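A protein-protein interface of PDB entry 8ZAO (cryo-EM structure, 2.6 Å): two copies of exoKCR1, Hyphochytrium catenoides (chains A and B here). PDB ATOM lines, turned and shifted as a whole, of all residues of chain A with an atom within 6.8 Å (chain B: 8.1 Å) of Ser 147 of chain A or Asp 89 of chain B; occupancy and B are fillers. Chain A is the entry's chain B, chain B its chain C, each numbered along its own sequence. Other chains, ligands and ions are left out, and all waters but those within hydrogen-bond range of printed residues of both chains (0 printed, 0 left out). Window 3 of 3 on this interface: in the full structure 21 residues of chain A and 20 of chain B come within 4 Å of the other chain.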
ATOM      1  N   ALA A 142      -5.824  -8.552   0.850  1.00  0.00           N
ATOM      2  CA  ALA A 142      -4.389  -8.574   0.585  1.00  0.00           C
ATOM      3  C   ALA A 142      -4.014  -7.635  -0.550  1.00  0.00           C
ATOM      4  O   ALA A 142      -2.939  -7.026  -0.521  1.00  0.00           O
ATOM      5  CB  ALA A 142      -3.933  -9.996   0.267  1.00  0.00           C
ATOM      6  N   VAL A 144      -5.639  -4.828  -1.388  1.00  0.00           N
ATOM      7  CA  VAL A 144      -5.810  -3.422  -1.024  1.00  0.00           C
ATOM      8  C   VAL A 144      -4.931  -3.000   0.144  1.00  0.00           C
ATOM      9  O   VAL A 144      -4.888  -1.804   0.472  1.00  0.00           O
ATOM     10  CB  VAL A 144      -7.277  -3.090  -0.688  1.00  0.00           C
ATOM     11  CG1 VAL A 144      -8.179  -3.428  -1.864  1.00  0.00           C
ATOM     12  CG2 VAL A 144      -7.713  -3.816   0.564  1.00  0.00           C
ATOM     13  N   THR A 145      -4.231  -3.935   0.784  1.00  0.00           N
ATOM     14  CA  THR A 145      -3.379  -3.613   1.922  1.00  0.00           C
ATOM     15  C   THR A 145      -1.977  -3.273   1.437  1.00  0.00           C
ATOM     16  O   THR A 145      -1.355  -4.098   0.754  1.00  0.00           O
ATOM     17  CB  THR A 145      -3.319  -4.777   2.895  1.00  0.00           C
ATOM     18  OG1 THR A 145      -4.641  -5.083   3.353  1.00  0.00           O
ATOM     19  CG2 THR A 145      -2.450  -4.426   4.088  1.00  0.00           C
ATOM     20  N   PRO A 146      -1.444  -2.090   1.752  1.00  0.00           N
ATOM     21  CA  PRO A 146      -0.111  -1.717   1.269  1.00  0.00           C
ATOM     22  C   PRO A 146       1.048  -2.153   2.151  1.00  0.00           C
ATOM     23  O   PRO A 146       2.202  -2.025   1.721  1.00  0.00           O
ATOM     24  CB  PRO A 146      -0.196  -0.186   1.218  1.00  0.00           C
ATOM     25  CG  PRO A 146      -1.140   0.163   2.319  1.00  0.00           C
ATOM     26  CD  PRO A 146      -2.098  -0.990   2.481  1.00  0.00           C
ATOM     27  N   SER A 147       0.787  -2.658   3.353  1.00  0.00           N
ATOM     28  CA  SER A 147       1.848  -3.042   4.271  1.00  0.00           C
ATOM     29  C   SER A 147       2.198  -4.515   4.072  1.00  0.00           C
ATOM     30  O   SER A 147       1.731  -5.169   3.136  1.00  0.00           O
ATOM     31  CB  SER A 147       1.431  -2.751   5.710  1.00  0.00           C
ATOM     32  OG  SER A 147       0.113  -3.206   5.959  1.00  0.00           O
ATOM     33  N   ALA A 148       3.035  -5.052   4.956  1.00  0.00           N
ATOM     34  CA  ALA A 148       3.375  -6.469   4.941  1.00  0.00           C
ATOM     35  C   ALA A 148       2.226  -7.348   5.408  1.00  0.00           C
ATOM     36  O   ALA A 148       2.205  -8.544   5.090  1.00  0.00           O
ATOM     37  CB  ALA A 148       4.610  -6.724   5.808  1.00  0.00           C
ATOM     38  N   TYR A 149       1.262  -6.782   6.128  1.00  0.00           N
ATOM     39  CA  TYR A 149       0.117  -7.530   6.625  1.00  0.00           C
ATOM     40  C   TYR A 149      -0.763  -8.061   5.506  1.00  0.00           C
ATOM     41  O   TYR A 149      -1.613  -8.920   5.763  1.00  0.00           O
ATOM     42  CB  TYR A 149      -0.712  -6.660   7.573  1.00  0.00           C
ATOM     43  CG  TYR A 149      -0.115  -6.555   8.954  1.00  0.00           C
ATOM     44  CD1 TYR A 149      -0.417  -7.490   9.933  1.00  0.00           C
ATOM     45  CD2 TYR A 149       0.762  -5.530   9.275  1.00  0.00           C
ATOM     46  CE1 TYR A 149       0.131  -7.401  11.195  1.00  0.00           C
ATOM     47  CE2 TYR A 149       1.314  -5.434  10.532  1.00  0.00           C
ATOM     48  CZ  TYR A 149       0.997  -6.371  11.489  1.00  0.00           C
ATOM     49  OH  TYR A 149       1.547  -6.275  12.746  1.00  0.00           O
ATOM     50  N   ARG A 150      -0.581  -7.577   4.277  1.00  0.00           N
ATOM     51  CA  ARG A 150      -1.220  -8.209   3.135  1.00  0.00           C
ATOM     52  C   ARG A 150      -0.820  -9.671   3.003  1.00  0.00           C
ATOM     53  O   ARG A 150      -1.684 -10.513   2.736  1.00  0.00           O
ATOM     54  CB  ARG A 150      -0.893  -7.437   1.849  1.00  0.00           C
ATOM     55  CG  ARG A 150       0.519  -7.618   1.315  1.00  0.00           C
ATOM     56  CD  ARG A 150       0.799  -6.702   0.140  1.00  0.00           C
ATOM     57  NE  ARG A 150       2.163  -6.855  -0.348  1.00  0.00           N
ATOM     58  CZ  ARG A 150       3.166  -6.046  -0.039  1.00  0.00           C
ATOM     59  NH1 ARG A 150       2.996  -5.008   0.762  1.00  0.00           N
ATOM     60  NH2 ARG A 150       4.373  -6.284  -0.546  1.00  0.00           N
ATOM     61  N   PHE A 151       0.456  -9.999   3.233  1.00  0.00           N
ATOM     62  CA  PHE A 151       0.870 -11.392   3.266  1.00  0.00           C
ATOM     63  C   PHE A 151       0.202 -12.159   4.394  1.00  0.00           C
ATOM     64  O   PHE A 151       0.086 -13.385   4.309  1.00  0.00           O
ATOM     65  CB  PHE A 151       2.389 -11.489   3.392  1.00  0.00           C
ATOM     66  CG  PHE A 151       3.129 -10.793   2.291  1.00  0.00           C
ATOM     67  CD1 PHE A 151       2.890 -11.118   0.968  1.00  0.00           C
ATOM     68  CD2 PHE A 151       4.057  -9.809   2.576  1.00  0.00           C
ATOM     69  CE1 PHE A 151       3.566 -10.478  -0.049  1.00  0.00           C
ATOM     70  CE2 PHE A 151       4.736  -9.166   1.564  1.00  0.00           C
ATOM     71  CZ  PHE A 151       4.490  -9.502   0.249  1.00  0.00           C
ATOM     72  N   ARG B   6      -4.882   6.538   8.579  1.00  0.00           N
ATOM     73  CA  ARG B   6      -4.074   6.942   9.719  1.00  0.00           C
ATOM     74  C   ARG B   6      -3.069   8.001   9.279  1.00  0.00           C
ATOM     75  O   ARG B   6      -2.366   7.802   8.281  1.00  0.00           O
ATOM     76  CB  ARG B   6      -3.353   5.743  10.325  1.00  0.00           C
ATOM     77  CG  ARG B   6      -2.627   6.057  11.622  1.00  0.00           C
ATOM     78  CD  ARG B   6      -1.859   4.854  12.133  1.00  0.00           C
ATOM     79  NE  ARG B   6      -0.948   4.326  11.128  1.00  0.00           N
ATOM     80  CZ  ARG B   6       0.295   4.748  10.950  1.00  0.00           C
ATOM     81  NH1 ARG B   6       0.815   5.703  11.703  1.00  0.00           N
ATOM     82  NH2 ARG B   6       1.037   4.198   9.993  1.00  0.00           N
ATOM     83  N   TRP B  11      -2.277   8.572  14.810  1.00  0.00           N
ATOM     84  CA  TRP B  11      -3.575   9.106  15.189  1.00  0.00           C
ATOM     85  C   TRP B  11      -3.394  10.269  16.161  1.00  0.00           C
ATOM     86  O   TRP B  11      -2.558  10.194  17.068  1.00  0.00           O
ATOM     87  CB  TRP B  11      -4.440   8.017  15.825  1.00  0.00           C
ATOM     88  CG  TRP B  11      -4.856   6.948  14.869  1.00  0.00           C
ATOM     89  CD1 TRP B  11      -4.462   5.643  14.878  1.00  0.00           C
ATOM     90  CD2 TRP B  11      -5.748   7.088  13.757  1.00  0.00           C
ATOM     91  NE1 TRP B  11      -5.053   4.962  13.843  1.00  0.00           N
ATOM     92  CE2 TRP B  11      -5.848   5.828  13.140  1.00  0.00           C
ATOM     93  CE3 TRP B  11      -6.472   8.158  13.226  1.00  0.00           C
ATOM     94  CZ2 TRP B  11      -6.641   5.608  12.019  1.00  0.00           C
ATOM     95  CZ3 TRP B  11      -7.259   7.938  12.113  1.00  0.00           C
ATOM     96  CH2 TRP B  11      -7.336   6.673  11.521  1.00  0.00           C
ATOM     97  N   TYR B  21      -3.539  -0.308  20.432  1.00  0.00           N
ATOM     98  CA  TYR B  21      -3.680  -1.171  19.267  1.00  0.00           C
ATOM     99  C   TYR B  21      -3.025  -2.541  19.437  1.00  0.00           C
ATOM    100  O   TYR B  21      -3.587  -3.531  18.957  1.00  0.00           O
ATOM    101  CB  TYR B  21      -3.136  -0.464  18.024  1.00  0.00           C
ATOM    102  CG  TYR B  21      -4.087   0.582  17.489  1.00  0.00           C
ATOM    103  CD1 TYR B  21      -5.248   0.213  16.828  1.00  0.00           C
ATOM    104  CD2 TYR B  21      -3.831   1.935  17.655  1.00  0.00           C
ATOM    105  CE1 TYR B  21      -6.123   1.160  16.341  1.00  0.00           C
ATOM    106  CE2 TYR B  21      -4.701   2.890  17.172  1.00  0.00           C
ATOM    107  CZ  TYR B  21      -5.845   2.496  16.515  1.00  0.00           C
ATOM    108  OH  TYR B  21      -6.718   3.440  16.029  1.00  0.00           O
ATOM    109  N   PRO B  22      -1.847  -2.664  20.062  1.00  0.00           N
ATOM    110  CA  PRO B  22      -1.343  -4.021  20.346  1.00  0.00           C
ATOM    111  C   PRO B  22      -2.282  -4.842  21.215  1.00  0.00           C
ATOM    112  O   PRO B  22      -2.492  -6.032  20.946  1.00  0.00           O
ATOM    113  CB  PRO B  22      -0.005  -3.751  21.044  1.00  0.00           C
ATOM    114  CG  PRO B  22       0.435  -2.457  20.488  1.00  0.00           C
ATOM    115  CD  PRO B  22      -0.818  -1.645  20.347  1.00  0.00           C
ATOM    116  N   GLY B  25      -5.323  -5.798  19.109  1.00  0.00           N
ATOM    117  CA  GLY B  25      -4.921  -6.825  18.167  1.00  0.00           C
ATOM    118  C   GLY B  25      -4.775  -8.186  18.811  1.00  0.00           C
ATOM    119  O   GLY B  25      -5.207  -9.191  18.243  1.00  0.00           O
ATOM    120  N   ALA B  82      -8.942 -10.657  10.465  1.00  0.00           N
ATOM    121  CA  ALA B  82      -8.760  -9.409   9.729  1.00  0.00           C
ATOM    122  C   ALA B  82      -8.734  -8.205  10.665  1.00  0.00           C
ATOM    123  O   ALA B  82      -7.964  -7.264  10.444  1.00  0.00           O
ATOM    124  CB  ALA B  82      -9.863  -9.249   8.686  1.00  0.00           C
ATOM    125  N   LYS B  83      -9.573  -8.214  11.703  1.00  0.00           N
ATOM    126  CA  LYS B  83      -9.568  -7.140  12.690  1.00  0.00           C
ATOM    127  C   LYS B  83      -8.244  -7.066  13.436  1.00  0.00           C
ATOM    128  O   LYS B  83      -7.743  -5.968  13.698  1.00  0.00           O
ATOM    129  CB  LYS B  83     -10.714  -7.336  13.680  1.00  0.00           C
ATOM    130  CG  LYS B  83     -12.089  -7.037  13.120  1.00  0.00           C
ATOM    131  CD  LYS B  83     -13.173  -7.488  14.079  1.00  0.00           C
ATOM    132  CE  LYS B  83     -14.545  -7.417  13.438  1.00  0.00           C
ATOM    133  NZ  LYS B  83     -15.326  -6.264  13.956  1.00  0.00           N
ATOM    134  N   SER B  84      -7.675  -8.214  13.805  1.00  0.00           N
ATOM    135  CA  SER B  84      -6.370  -8.226  14.453  1.00  0.00           C
ATOM    136  C   SER B  84      -5.287  -7.727  13.508  1.00  0.00           C
ATOM    137  O   SER B  84      -4.362  -7.027  13.932  1.00  0.00           O
ATOM    138  CB  SER B  84      -6.040  -9.630  14.955  1.00  0.00           C
ATOM    139  OG  SER B  84      -6.117 -10.577  13.905  1.00  0.00           O
ATOM    140  N   PHE B  85      -5.377  -8.087  12.226  1.00  0.00           N
ATOM    141  CA  PHE B  85      -4.431  -7.554  11.248  1.00  0.00           C
ATOM    142  C   PHE B  85      -4.537  -6.037  11.155  1.00  0.00           C
ATOM    143  O   PHE B  85      -3.519  -5.340  11.077  1.00  0.00           O
ATOM    144  CB  PHE B  85      -4.670  -8.187   9.877  1.00  0.00           C
ATOM    145  CG  PHE B  85      -4.476  -9.675   9.846  1.00  0.00           C
ATOM    146  CD1 PHE B  85      -3.697 -10.309  10.799  1.00  0.00           C
ATOM    147  CD2 PHE B  85      -5.075 -10.441   8.863  1.00  0.00           C
ATOM    148  CE1 PHE B  85      -3.521 -11.677  10.769  1.00  0.00           C
ATOM    149  CE2 PHE B  85      -4.902 -11.808   8.829  1.00  0.00           C
ATOM    150  CZ  PHE B  85      -4.126 -12.427   9.782  1.00  0.00           C
ATOM    151  N   ASP B  86      -5.763  -5.513  11.150  1.00  0.00           N
ATOM    152  CA  ASP B  86      -5.962  -4.069  11.092  1.00  0.00           C
ATOM    153  C   ASP B  86      -5.430  -3.379  12.343  1.00  0.00           C
ATOM    154  O   ASP B  86      -4.786  -2.328  12.254  1.00  0.00           O
ATOM    155  CB  ASP B  86      -7.447  -3.760  10.898  1.00  0.00           C
ATOM    156  CG  ASP B  86      -7.808  -2.350  11.312  1.00  0.00           C
ATOM    157  OD1 ASP B  86      -7.546  -1.413  10.532  1.00  0.00           O
ATOM    158  OD2 ASP B  86      -8.363  -2.176  12.417  1.00  0.00           O
ATOM    159  N   PHE B  87      -5.695  -3.953  13.517  1.00  0.00           N
ATOM    160  CA  PHE B  87      -5.267  -3.333  14.767  1.00  0.00           C
ATOM    161  C   PHE B  87      -3.753  -3.377  14.923  1.00  0.00           C
ATOM    162  O   PHE B  87      -3.141  -2.401  15.372  1.00  0.00           O
ATOM    163  CB  PHE B  87      -5.947  -4.018  15.949  1.00  0.00           C
ATOM    164  CG  PHE B  87      -7.325  -3.503  16.237  1.00  0.00           C
ATOM    165  CD1 PHE B  87      -7.650  -2.183  15.983  1.00  0.00           C
ATOM    166  CD2 PHE B  87      -8.296  -4.339  16.758  1.00  0.00           C
ATOM    167  CE1 PHE B  87      -8.915  -1.705  16.246  1.00  0.00           C
ATOM    168  CE2 PHE B  87      -9.563  -3.866  17.023  1.00  0.00           C
ATOM    169  CZ  PHE B  87      -9.872  -2.548  16.768  1.00  0.00           C
ATOM    170  N   PHE B  88      -3.132  -4.502  14.566  1.00  0.00           N
ATOM    171  CA  PHE B  88      -1.684  -4.625  14.664  1.00  0.00           C
ATOM    172  C   PHE B  88      -0.961  -3.712  13.686  1.00  0.00           C
ATOM    173  O   PHE B  88       0.216  -3.406  13.896  1.00  0.00           O
ATOM    174  CB  PHE B  88      -1.268  -6.076  14.433  1.00  0.00           C
ATOM    175  CG  PHE B  88      -1.326  -6.924  15.669  1.00  0.00           C
ATOM    176  CD1 PHE B  88      -0.798  -6.467  16.863  1.00  0.00           C
ATOM    177  CD2 PHE B  88      -1.913  -8.176  15.638  1.00  0.00           C
ATOM    178  CE1 PHE B  88      -0.850  -7.243  17.999  1.00  0.00           C
ATOM    179  CE2 PHE B  88      -1.970  -8.956  16.772  1.00  0.00           C
ATOM    180  CZ  PHE B  88      -1.437  -8.489  17.954  1.00  0.00           C
ATOM    181  N   ASP B  89      -1.637  -3.273  12.628  1.00  0.00           N
ATOM    182  CA  ASP B  89      -1.081  -2.313  11.687  1.00  0.00           C
ATOM    183  C   ASP B  89      -1.298  -0.872  12.125  1.00  0.00           C
ATOM    184  O   ASP B  89      -0.883   0.046  11.412  1.00  0.00           O
ATOM    185  CB  ASP B  89      -1.687  -2.530  10.298  1.00  0.00           C
ATOM    186  CG  ASP B  89      -0.735  -2.154   9.181  1.00  0.00           C
ATOM    187  OD1 ASP B  89       0.416  -1.777   9.481  1.00  0.00           O
ATOM    188  OD2 ASP B  89      -1.136  -2.242   8.003  1.00  0.00           O
ATOM    189  N   GLY B  90      -1.936  -0.654  13.270  1.00  0.00           N
ATOM    190  CA  GLY B  90      -2.162   0.677  13.786  1.00  0.00           C
ATOM    191  C   GLY B  90      -3.521   1.271  13.497  1.00  0.00           C
ATOM    192  O   GLY B  90      -3.750   2.434  13.841  1.00  0.00           O
ATOM    193  N   GLY B  91      -4.423   0.519  12.883  1.00  0.00           N
ATOM    194  CA  GLY B  91      -5.740   1.019  12.562  1.00  0.00           C
ATOM    195  C   GLY B  91      -5.745   1.882  11.312  1.00  0.00           C
ATOM    196  O   GLY B  91      -4.708   2.300  10.798  1.00  0.00           O
ATOM    197  N   GLY B  92      -6.950   2.153  10.821  1.00  0.00           N
ATOM    198  CA  GLY B  92      -7.098   2.954   9.621  1.00  0.00           C
ATOM    199  C   GLY B  92      -6.591   2.289   8.362  1.00  0.00           C
ATOM    200  O   GLY B  92      -6.338   2.974   7.367  1.00  0.00           O
ATOM    201  N   THR B  93      -6.433   0.969   8.380  1.00  0.00           N
ATOM    202  CA  THR B  93      -6.020   0.092   7.292  1.00  0.00           C
ATOM    203  C   THR B  93      -7.077   0.104   6.191  1.00  0.00           C
ATOM    204  O   THR B  93      -8.273   0.111   6.488  1.00  0.00           O
ATOM    205  CB  THR B  93      -5.817  -1.332   7.810  1.00  0.00           C
ATOM    206  OG1 THR B  93      -4.650  -1.374   8.639  1.00  0.00           O
ATOM    207  CG2 THR B  93      -5.656  -2.328   6.671  1.00  0.00           C
ATOM    208  N   PRO B  94      -6.666   0.137   4.911  1.00  0.00           N
ATOM    209  CA  PRO B  94      -7.646   0.200   3.815  1.00  0.00           C
ATOM    210  C   PRO B  94      -8.759  -0.833   3.918  1.00  0.00           C
ATOM    211  O   PRO B  94      -9.932  -0.499   3.727  1.00  0.00           O
ATOM    212  CB  PRO B  94      -6.783  -0.037   2.573  1.00  0.00           C
ATOM    213  CG  PRO B  94      -5.451   0.509   2.941  1.00  0.00           C
ATOM    214  CD  PRO B  94      -5.293   0.379   4.435  1.00  0.00           C
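Of the 18 printed residues of chain B, 4 touch a printed residue of chain A. Hydrophobic or aromatic side chains of chain B that line the printed part of chain A: Phe 88 and Pro 94. Of the 9 printed residues of chain A, 4 touch a printed residue of chain B. Among the printed residues, 6 pairs touch across the chains.
Ser 147 of chain A touches one residue of chain B. Pro 146 of chain A touches just one residue of chain B: Pro 94. No residue of chain B comes within 4 Å of Ala 148 of chain A. Printed residues of chain A within 4 Å of Phe 88 of chain B: Tyr 149. Of the printed residues of chain B, Tyr 149 of chain A touches Phe 85, Phe 88 and Asp 89. Of the printed residues of chain A, Pro 94 of chain B touches Val 144 and Pro 146.
No position is printed for both chains.
Among the printed residues, merely in contact across the chains: Val 144 of chain A with Pro 94 of chain B (3.3 Å), Tyr 149 of chain A with Asp 89 of chain B (3.7 Å), Pro 146 of chain A with Pro 94 of chain B (3.7 Å) and Tyr 149 of chain A with Phe 85 of chain B (3.9 Å).
The guanidinium group (NH1) of Arg 150 of chain A lies within hydrogen-bond range of the backbone carbonyl oxygen (O) of Pro 146 of chain A (3.2 Å). The backbone carbonyl oxygen (O) of Ser 147 of chain A sits at hydrogen-bond distance from the guanidinium group (NH1) of Arg 150 of chain A, at 2.7 Å.
OD2 of Asp 89 of chain B is in hydrogen-bond range of OG of Ser 147 of chain A, 2.6 Å away. The side-chain hydroxyl of Tyr 149 of chain A lies close to the backbone carbonyl oxygen of Phe 88 of chain B, at 3.4 Å.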
